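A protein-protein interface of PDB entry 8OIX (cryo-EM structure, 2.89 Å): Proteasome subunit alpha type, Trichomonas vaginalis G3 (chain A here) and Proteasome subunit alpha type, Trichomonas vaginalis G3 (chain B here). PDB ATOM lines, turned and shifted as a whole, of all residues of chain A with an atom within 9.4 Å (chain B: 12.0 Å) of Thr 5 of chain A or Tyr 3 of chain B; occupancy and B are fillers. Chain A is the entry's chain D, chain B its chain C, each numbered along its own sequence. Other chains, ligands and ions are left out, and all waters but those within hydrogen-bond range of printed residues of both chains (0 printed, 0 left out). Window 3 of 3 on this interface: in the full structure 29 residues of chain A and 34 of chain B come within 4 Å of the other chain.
OH of Tyr 3 of chain B sits at hydrogen-bond distance from O of Thr 5 of chain A (2.6 Å). The side-chain hydroxyl of Tyr 4 of chain A is in hydrogen-bond range of the side-chain carboxylate of Asp 6 of chain B. The guanidinium group (NE) of Arg 6 of chain A lies within salt-bridge range of the side-chain carboxylate (OD2) of Asp 6 of chain B, 2.9 Å away. OG1 of Thr 11 of chain B sits at hydrogen-bond distance from NH1 of Arg 6 of chain A, at 2.9 Å. O of Gly 124 of chain A lies within hydrogen-bond range of N of Gly 124 of chain B, at 3.3 Å.
N of Gly 8 of chain B sits at hydrogen-bond distance from OD2 of Asp 6 of chain B, 3.2 Å away. The backbone carbonyl oxygen (O) of Gly 125 of chain B sits close to the side-chain hydroxyl (OG1) of Thr 9 of chain B (3.1 Å).
Among the printed residues, pairs that only touch across the chains: Tyr 4 of chain A with Gly 124 of chain B, Tyr 4 of chain A with Gly 125 of chain B, Ile 8 of chain A with Thr 11 of chain B, Gly 124 of chain A with Tyr 123 of chain B, Ile 8 of chain A with Thr 10 of chain B, Ala 125 of chain A with Gln 122 of chain B, Arg 6 of chain A with Tyr 3 of chain B, Ala 125 of chain A with Tyr 123 of chain B, Gly 124 of chain A with Gln 122 of chain B, Tyr 4 of chain A with Tyr 3 of chain B and Tyr 4 of chain A with Thr 10 of chain B.
Thr 5 of chain A touches just one residue of chain B: Tyr 3 (2.6 Å). Tyr 3 of chain B touches three residues of chain A. No residue of chain B comes within 4 Å of Asp 3 of chain A. Tyr 4 of chain A touches just these residues of chain B: Tyr 3 (3.7 Å), Asp 6 (3.2 Å), Thr 10 (3.8 Å), Gly 124 (3.2 Å) and Gly 125 (3.2 Å). Arg 6 of chain A touches three residues of chain B. No residue of chain B comes within 4 Å of Ser 7 of chain A. Printed residues of chain B within 4 Å of Gly 124 of chain A: Gln 122, Tyr 123 and Gly 124. No residue of chain A comes within 4 Å of Thr 2 of chain B. Asp 6 of chain B touches two residues of chain A. Printed residues of chain A within 4 Å of Gly 125 of chain B: Tyr 4. Printed residues of chain A within 4 Å of Gln 122 of chain B: Gly 124 (3.7 Å) and Ala 125 (3.4 Å). Ala 7 of chain B touches none of the printed residues of chain A. Gln 121 of chain A touches none of the printed residues of chain B. The nearest residue of chain B that does not touch Thr 5 of chain A is Gly 124 of chain B (6.5 Å). The nearest residue of chain A that does not touch Tyr 3 of chain B is Asp 3 of chain A (5.5 Å).
Of the 13 printed residues of chain A, 6 touch a printed residue of chain B. Among the printed residues, 16 pairs touch across the chains.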
ATOM      1  N   ASP A   3       4.790 -29.042 -33.050  1.00  0.00           N
ATOM      2  CA  ASP A   3       5.327 -29.856 -31.968  1.00  0.00           C
ATOM      3  C   ASP A   3       5.904 -28.966 -30.868  1.00  0.00           C
ATOM      4  O   ASP A   3       5.956 -27.744 -31.005  1.00  0.00           O
ATOM      5  CB  ASP A   3       6.392 -30.821 -32.496  1.00  0.00           C
ATOM      6  CG  ASP A   3       6.568 -32.042 -31.609  1.00  0.00           C
ATOM      7  OD1 ASP A   3       6.384 -31.921 -30.380  1.00  0.00           O
ATOM      8  OD2 ASP A   3       6.887 -33.125 -32.143  1.00  0.00           O
ATOM      9  N   TYR A   4       6.329 -29.594 -29.775  1.00  0.00           N
ATOM     10  CA  TYR A   4       6.848 -28.864 -28.626  1.00  0.00           C
ATOM     11  C   TYR A   4       8.194 -28.227 -28.955  1.00  0.00           C
ATOM     12  O   TYR A   4       9.108 -28.898 -29.443  1.00  0.00           O
ATOM     13  CB  TYR A   4       6.981 -29.832 -27.455  1.00  0.00           C
ATOM     14  CG  TYR A   4       7.538 -29.285 -26.163  1.00  0.00           C
ATOM     15  CD1 TYR A   4       6.725 -28.617 -25.262  1.00  0.00           C
ATOM     16  CD2 TYR A   4       8.867 -29.487 -25.819  1.00  0.00           C
ATOM     17  CE1 TYR A   4       7.229 -28.138 -24.072  1.00  0.00           C
ATOM     18  CE2 TYR A   4       9.379 -29.010 -24.630  1.00  0.00           C
ATOM     19  CZ  TYR A   4       8.550 -28.346 -23.756  1.00  0.00           C
ATOM     20  OH  TYR A   4       9.049 -27.869 -22.567  1.00  0.00           O
ATOM     21  N   THR A   5       8.313 -26.921 -28.678  1.00  0.00           N
ATOM     22  CA  THR A   5       9.527 -26.135 -28.907  1.00  0.00           C
ATOM     23  C   THR A   5       9.656 -25.114 -27.774  1.00  0.00           C
ATOM     24  O   THR A   5       9.272 -23.952 -27.890  1.00  0.00           O
ATOM     25  CB  THR A   5       9.516 -25.429 -30.265  1.00  0.00           C
ATOM     26  OG1 THR A   5       8.324 -24.643 -30.389  1.00  0.00           O
ATOM     27  CG2 THR A   5       9.591 -26.425 -31.408  1.00  0.00           C
ATOM     28  N   ARG A   6      10.214 -25.543 -26.643  1.00  0.00           N
ATOM     29  CA  ARG A   6      10.330 -24.681 -25.475  1.00  0.00           C
ATOM     30  C   ARG A   6      11.747 -24.147 -25.298  1.00  0.00           C
ATOM     31  O   ARG A   6      12.058 -23.560 -24.258  1.00  0.00           O
ATOM     32  CB  ARG A   6       9.869 -25.448 -24.232  1.00  0.00           C
ATOM     33  CG  ARG A   6       9.808 -24.697 -22.897  1.00  0.00           C
ATOM     34  CD  ARG A   6      10.891 -25.189 -21.944  1.00  0.00           C
ATOM     35  NE  ARG A   6      10.767 -24.624 -20.606  1.00  0.00           N
ATOM     36  CZ  ARG A   6      11.598 -24.885 -19.606  1.00  0.00           C
ATOM     37  NH1 ARG A   6      12.657 -25.660 -19.772  1.00  0.00           N
ATOM     38  NH2 ARG A   6      11.369 -24.342 -18.413  1.00  0.00           N
ATOM     39  N   SER A   7      12.583 -24.258 -26.326  1.00  0.00           N
ATOM     40  CA  SER A   7      13.951 -23.746 -26.294  1.00  0.00           C
ATOM     41  C   SER A   7      14.602 -24.056 -24.948  1.00  0.00           C
ATOM     42  O   SER A   7      14.918 -23.168 -24.157  1.00  0.00           O
ATOM     43  CB  SER A   7      13.986 -22.250 -26.585  1.00  0.00           C
ATOM     44  OG  SER A   7      15.322 -21.782 -26.608  1.00  0.00           O
ATOM     45  N   ILE A   8      14.739 -25.354 -24.675  1.00  0.00           N
ATOM     46  CA  ILE A   8      15.316 -25.803 -23.410  1.00  0.00           C
ATOM     47  C   ILE A   8      16.661 -25.134 -23.166  1.00  0.00           C
ATOM     48  O   ILE A   8      16.959 -24.690 -22.050  1.00  0.00           O
ATOM     49  CB  ILE A   8      15.428 -27.341 -23.386  1.00  0.00           C
ATOM     50  CG1 ILE A   8      14.088 -27.989 -23.015  1.00  0.00           C
ATOM     51  CG2 ILE A   8      16.513 -27.794 -22.431  1.00  0.00           C
ATOM     52  CD1 ILE A   8      13.011 -27.879 -24.062  1.00  0.00           C
ATOM     53  N   THR A   9      17.480 -25.023 -24.205  1.00  0.00           N
ATOM     54  CA  THR A   9      18.814 -24.450 -24.092  1.00  0.00           C
ATOM     55  C   THR A   9      18.751 -22.975 -24.469  1.00  0.00           C
ATOM     56  O   THR A   9      18.556 -22.633 -25.640  1.00  0.00           O
ATOM     57  CB  THR A   9      19.802 -25.192 -24.987  1.00  0.00           C
ATOM     58  OG1 THR A   9      19.850 -26.568 -24.602  1.00  0.00           O
ATOM     59  CG2 THR A   9      21.190 -24.594 -24.850  1.00  0.00           C
ATOM     60  N   ARG A  10      18.917 -22.104 -23.478  1.00  0.00           N
ATOM     61  CA  ARG A  10      18.951 -20.668 -23.697  1.00  0.00           C
ATOM     62  C   ARG A  10      20.171 -20.103 -22.994  1.00  0.00           C
ATOM     63  O   ARG A  10      20.722 -20.711 -22.074  1.00  0.00           O
ATOM     64  CB  ARG A  10      17.699 -19.951 -23.167  1.00  0.00           C
ATOM     65  CG  ARG A  10      16.421 -20.738 -23.261  1.00  0.00           C
ATOM     66  CD  ARG A  10      15.231 -19.923 -22.788  1.00  0.00           C
ATOM     67  NE  ARG A  10      15.515 -19.204 -21.554  1.00  0.00           N
ATOM     68  CZ  ARG A  10      15.456 -17.886 -21.424  1.00  0.00           C
ATOM     69  NH1 ARG A  10      15.406 -17.090 -22.479  1.00  0.00           N
ATOM     70  NH2 ARG A  10      15.537 -17.351 -20.210  1.00  0.00           N
ATOM     71  N   GLN A 121      20.378 -26.758 -29.906  1.00  0.00           N
ATOM     72  CA  GLN A 121      19.787 -25.720 -30.741  1.00  0.00           C
ATOM     73  C   GLN A 121      18.322 -25.949 -31.057  1.00  0.00           C
ATOM     74  O   GLN A 121      17.604 -24.982 -31.311  1.00  0.00           O
ATOM     75  CB  GLN A 121      20.558 -25.591 -32.061  1.00  0.00           C
ATOM     76  CG  GLN A 121      21.980 -25.081 -31.918  1.00  0.00           C
ATOM     77  CD  GLN A 121      22.728 -25.077 -33.237  1.00  0.00           C
ATOM     78  OE1 GLN A 121      22.351 -25.772 -34.180  1.00  0.00           O
ATOM     79  NE2 GLN A 121      23.786 -24.280 -33.314  1.00  0.00           N
ATOM     80  N   SER A 122      17.863 -27.197 -31.074  1.00  0.00           N
ATOM     81  CA  SER A 122      16.484 -27.485 -31.434  1.00  0.00           C
ATOM     82  C   SER A 122      15.578 -27.234 -30.238  1.00  0.00           C
ATOM     83  O   SER A 122      15.851 -27.708 -29.130  1.00  0.00           O
ATOM     84  CB  SER A 122      16.341 -28.930 -31.912  1.00  0.00           C
ATOM     85  OG  SER A 122      17.143 -29.170 -33.055  1.00  0.00           O
ATOM     86  N   GLY A 123      14.505 -26.481 -30.459  1.00  0.00           N
ATOM     87  CA  GLY A 123      13.534 -26.273 -29.407  1.00  0.00           C
ATOM     88  C   GLY A 123      12.831 -27.564 -29.037  1.00  0.00           C
ATOM     89  O   GLY A 123      12.574 -28.427 -29.877  1.00  0.00           O
ATOM     90  N   GLY A 124      12.518 -27.696 -27.752  1.00  0.00           N
ATOM     91  CA  GLY A 124      11.905 -28.919 -27.276  1.00  0.00           C
ATOM     92  C   GLY A 124      12.819 -30.120 -27.279  1.00  0.00           C
ATOM     93  O   GLY A 124      12.336 -31.253 -27.248  1.00  0.00           O
ATOM     94  N   ALA A 125      14.132 -29.906 -27.315  1.00  0.00           N
ATOM     95  CA  ALA A 125      15.108 -30.987 -27.346  1.00  0.00           C
ATOM     96  C   ALA A 125      16.108 -30.785 -26.219  1.00  0.00           C
ATOM     97  O   ALA A 125      16.717 -29.716 -26.111  1.00  0.00           O
ATOM     98  CB  ALA A 125      15.825 -31.046 -28.697  1.00  0.00           C
ATOM     99  N   THR B   2       4.310 -17.713 -23.009  1.00  0.00           N
ATOM    100  CA  THR B   2       3.824 -19.052 -22.696  1.00  0.00           C
ATOM    101  C   THR B   2       4.853 -19.844 -21.899  1.00  0.00           C
ATOM    102  O   THR B   2       5.850 -19.292 -21.434  1.00  0.00           O
ATOM    103  CB  THR B   2       3.463 -19.834 -23.971  1.00  0.00           C
ATOM    104  OG1 THR B   2       4.653 -20.104 -24.725  1.00  0.00           O
ATOM    105  CG2 THR B   2       2.493 -19.038 -24.824  1.00  0.00           C
ATOM    106  N   TYR B   3       4.585 -21.141 -21.737  1.00  0.00           N
ATOM    107  CA  TYR B   3       5.426 -22.070 -20.983  1.00  0.00           C
ATOM    108  C   TYR B   3       5.515 -21.706 -19.506  1.00  0.00           C
ATOM    109  O   TYR B   3       6.395 -22.201 -18.795  1.00  0.00           O
ATOM    110  CB  TYR B   3       6.835 -22.174 -21.581  1.00  0.00           C
ATOM    111  CG  TYR B   3       6.861 -22.723 -22.987  1.00  0.00           C
ATOM    112  CD1 TYR B   3       6.422 -24.011 -23.256  1.00  0.00           C
ATOM    113  CD2 TYR B   3       7.337 -21.958 -24.042  1.00  0.00           C
ATOM    114  CE1 TYR B   3       6.446 -24.518 -24.536  1.00  0.00           C
ATOM    115  CE2 TYR B   3       7.366 -22.458 -25.326  1.00  0.00           C
ATOM    116  CZ  TYR B   3       6.918 -23.737 -25.567  1.00  0.00           C
ATOM    117  OH  TYR B   3       6.944 -24.243 -26.843  1.00  0.00           O
ATOM    118  N   ARG B   4       4.619 -20.838 -19.029  1.00  0.00           N
ATOM    119  CA  ARG B   4       4.602 -20.505 -17.609  1.00  0.00           C
ATOM    120  C   ARG B   4       4.273 -21.727 -16.763  1.00  0.00           C
ATOM    121  O   ARG B   4       4.867 -21.934 -15.699  1.00  0.00           O
ATOM    122  CB  ARG B   4       3.602 -19.381 -17.341  1.00  0.00           C
ATOM    123  CG  ARG B   4       3.640 -18.863 -15.912  1.00  0.00           C
ATOM    124  CD  ARG B   4       2.616 -17.766 -15.677  1.00  0.00           C
ATOM    125  NE  ARG B   4       3.071 -16.477 -16.185  1.00  0.00           N
ATOM    126  CZ  ARG B   4       2.597 -15.305 -15.785  1.00  0.00           C
ATOM    127  NH1 ARG B   4       1.641 -15.219 -14.875  1.00  0.00           N
ATOM    128  NH2 ARG B   4       3.093 -14.190 -16.315  1.00  0.00           N
ATOM    129  N   TYR B   5       3.332 -22.552 -17.222  1.00  0.00           N
ATOM    130  CA  TYR B   5       2.906 -23.739 -16.495  1.00  0.00           C
ATOM    131  C   TYR B   5       3.531 -25.011 -17.054  1.00  0.00           C
ATOM    132  O   TYR B   5       2.975 -26.102 -16.895  1.00  0.00           O
ATOM    133  CB  TYR B   5       1.381 -23.833 -16.511  1.00  0.00           C
ATOM    134  CG  TYR B   5       0.727 -22.520 -16.163  1.00  0.00           C
ATOM    135  CD1 TYR B   5       0.916 -21.937 -14.919  1.00  0.00           C
ATOM    136  CD2 TYR B   5      -0.053 -21.846 -17.091  1.00  0.00           C
ATOM    137  CE1 TYR B   5       0.332 -20.728 -14.602  1.00  0.00           C
ATOM    138  CE2 TYR B   5      -0.640 -20.639 -16.785  1.00  0.00           C
ATOM    139  CZ  TYR B   5      -0.445 -20.084 -15.540  1.00  0.00           C
ATOM    140  OH  TYR B   5      -1.029 -18.878 -15.236  1.00  0.00           O
ATOM    141  N   ASP B   6       4.682 -24.887 -17.708  1.00  0.00           N
ATOM    142  CA  ASP B   6       5.423 -26.036 -18.200  1.00  0.00           C
ATOM    143  C   ASP B   6       6.344 -26.551 -17.103  1.00  0.00           C
ATOM    144  O   ASP B   6       6.930 -25.769 -16.349  1.00  0.00           O
ATOM    145  CB  ASP B   6       6.225 -25.658 -19.448  1.00  0.00           C
ATOM    146  CG  ASP B   6       7.298 -26.671 -19.785  1.00  0.00           C
ATOM    147  OD1 ASP B   6       6.962 -27.854 -19.987  1.00  0.00           O
ATOM    148  OD2 ASP B   6       8.481 -26.279 -19.854  1.00  0.00           O
ATOM    149  N   ALA B   7       6.467 -27.871 -17.015  1.00  0.00           N
ATOM    150  CA  ALA B   7       7.250 -28.498 -15.960  1.00  0.00           C
ATOM    151  C   ALA B   7       8.680 -28.803 -16.378  1.00  0.00           C
ATOM    152  O   ALA B   7       9.451 -29.310 -15.558  1.00  0.00           O
ATOM    153  CB  ALA B   7       6.568 -29.786 -15.492  1.00  0.00           C
ATOM    154  N   GLY B   8       9.059 -28.483 -17.613  1.00  0.00           N
ATOM    155  CA  GLY B   8      10.377 -28.816 -18.110  1.00  0.00           C
ATOM    156  C   GLY B   8      10.692 -30.291 -17.988  1.00  0.00           C
ATOM    157  O   GLY B   8      11.735 -30.670 -17.446  1.00  0.00           O
ATOM    158  N   THR B   9       9.784 -31.135 -18.483  1.00  0.00           N
ATOM    159  CA  THR B   9       9.971 -32.577 -18.372  1.00  0.00           C
ATOM    160  C   THR B   9      11.204 -33.029 -19.142  1.00  0.00           C
ATOM    161  O   THR B   9      11.888 -33.975 -18.737  1.00  0.00           O
ATOM    162  CB  THR B   9       8.731 -33.310 -18.875  1.00  0.00           C
ATOM    163  OG1 THR B   9       8.608 -33.123 -20.289  1.00  0.00           O
ATOM    164  CG2 THR B   9       7.492 -32.765 -18.199  1.00  0.00           C
ATOM    165  N   THR B  10      11.493 -32.377 -20.265  1.00  0.00           N
ATOM    166  CA  THR B  10      12.673 -32.667 -21.073  1.00  0.00           C
ATOM    167  C   THR B  10      13.750 -31.615 -20.853  1.00  0.00           C
ATOM    168  O   THR B  10      14.396 -31.153 -21.796  1.00  0.00           O
ATOM    169  CB  THR B  10      12.301 -32.757 -22.549  1.00  0.00           C
ATOM    170  OG1 THR B  10      11.663 -31.541 -22.954  1.00  0.00           O
ATOM    171  CG2 THR B  10      11.353 -33.919 -22.784  1.00  0.00           C
ATOM    172  N   THR B  11      13.939 -31.208 -19.601  1.00  0.00           N
ATOM    173  CA  THR B  11      14.920 -30.203 -19.232  1.00  0.00           C
ATOM    174  C   THR B  11      15.786 -30.738 -18.099  1.00  0.00           C
ATOM    175  O   THR B  11      15.314 -31.472 -17.228  1.00  0.00           O
ATOM    176  CB  THR B  11      14.233 -28.896 -18.805  1.00  0.00           C
ATOM    177  OG1 THR B  11      13.304 -28.495 -19.819  1.00  0.00           O
ATOM    178  CG2 THR B  11      15.247 -27.784 -18.601  1.00  0.00           C
ATOM    179  N   SER B 119      13.060 -41.018 -25.338  1.00  0.00           N
ATOM    180  CA  SER B 119      12.497 -39.972 -26.179  1.00  0.00           C
ATOM    181  C   SER B 119      11.506 -39.136 -25.390  1.00  0.00           C
ATOM    182  O   SER B 119      11.419 -37.918 -25.578  1.00  0.00           O
ATOM    183  CB  SER B 119      11.828 -40.589 -27.407  1.00  0.00           C
ATOM    184  OG  SER B 119      10.799 -41.485 -27.029  1.00  0.00           O
ATOM    185  N   GLN B 122      13.701 -36.686 -23.490  1.00  0.00           N
ATOM    186  CA  GLN B 122      14.570 -35.777 -24.227  1.00  0.00           C
ATOM    187  C   GLN B 122      13.849 -34.915 -25.250  1.00  0.00           C
ATOM    188  O   GLN B 122      14.377 -33.857 -25.612  1.00  0.00           O
ATOM    189  CB  GLN B 122      15.678 -36.560 -24.949  1.00  0.00           C
ATOM    190  CG  GLN B 122      16.820 -35.691 -25.454  1.00  0.00           C
ATOM    191  CD  GLN B 122      18.015 -36.494 -25.917  1.00  0.00           C
ATOM    192  OE1 GLN B 122      17.872 -37.606 -26.419  1.00  0.00           O
ATOM    193  NE2 GLN B 122      19.204 -35.934 -25.742  1.00  0.00           N
ATOM    194  N   TYR B 123      12.664 -35.303 -25.711  1.00  0.00           N
ATOM    195  CA  TYR B 123      11.966 -34.552 -26.741  1.00  0.00           C
ATOM    196  C   TYR B 123      10.494 -34.432 -26.376  1.00  0.00           C
ATOM    197  O   TYR B 123       9.944 -35.255 -25.643  1.00  0.00           O
ATOM    198  CB  TYR B 123      12.109 -35.219 -28.115  1.00  0.00           C
ATOM    199  CG  TYR B 123      13.539 -35.420 -28.558  1.00  0.00           C
ATOM    200  CD1 TYR B 123      14.243 -34.401 -29.185  1.00  0.00           C
ATOM    201  CD2 TYR B 123      14.185 -36.630 -28.349  1.00  0.00           C
ATOM    202  CE1 TYR B 123      15.549 -34.582 -29.591  1.00  0.00           C
ATOM    203  CE2 TYR B 123      15.492 -36.819 -28.750  1.00  0.00           C
ATOM    204  CZ  TYR B 123      16.170 -35.793 -29.371  1.00  0.00           C
ATOM    205  OH  TYR B 123      17.471 -35.979 -29.774  1.00  0.00           O
ATOM    206  N   GLY B 124       9.865 -33.380 -26.895  1.00  0.00           N
ATOM    207  CA  GLY B 124       8.427 -33.251 -26.871  1.00  0.00           C
ATOM    208  C   GLY B 124       7.844 -32.663 -25.607  1.00  0.00           C
ATOM    209  O   GLY B 124       6.639 -32.384 -25.575  1.00  0.00           O
ATOM    210  N   GLY B 125       8.652 -32.462 -24.567  1.00  0.00           N
ATOM    211  CA  GLY B 125       8.147 -31.882 -23.334  1.00  0.00           C
ATOM    212  C   GLY B 125       7.002 -32.643 -22.711  1.00  0.00           C
ATOM    213  O   GLY B 125       6.196 -32.053 -21.984  1.00  0.00           O
ATOM    214  N   LEU B 126       6.909 -33.941 -22.968  1.00  0.00           N
ATOM    215  CA  LEU B 126       5.846 -34.772 -22.427  1.00  0.00           C
ATOM    216  C   LEU B 126       6.307 -35.448 -21.144  1.00  0.00           C
ATOM    217  O   LEU B 126       7.493 -35.474 -20.810  1.00  0.00           O
ATOM    218  CB  LEU B 126       5.407 -35.821 -23.451  1.00  0.00           C
ATOM    219  CG  LEU B 126       4.832 -35.300 -24.766  1.00  0.00           C
ATOM    220  CD1 LEU B 126       4.331 -36.452 -25.619  1.00  0.00           C
ATOM    221  CD2 LEU B 126       3.719 -34.314 -24.492  1.00  0.00           C
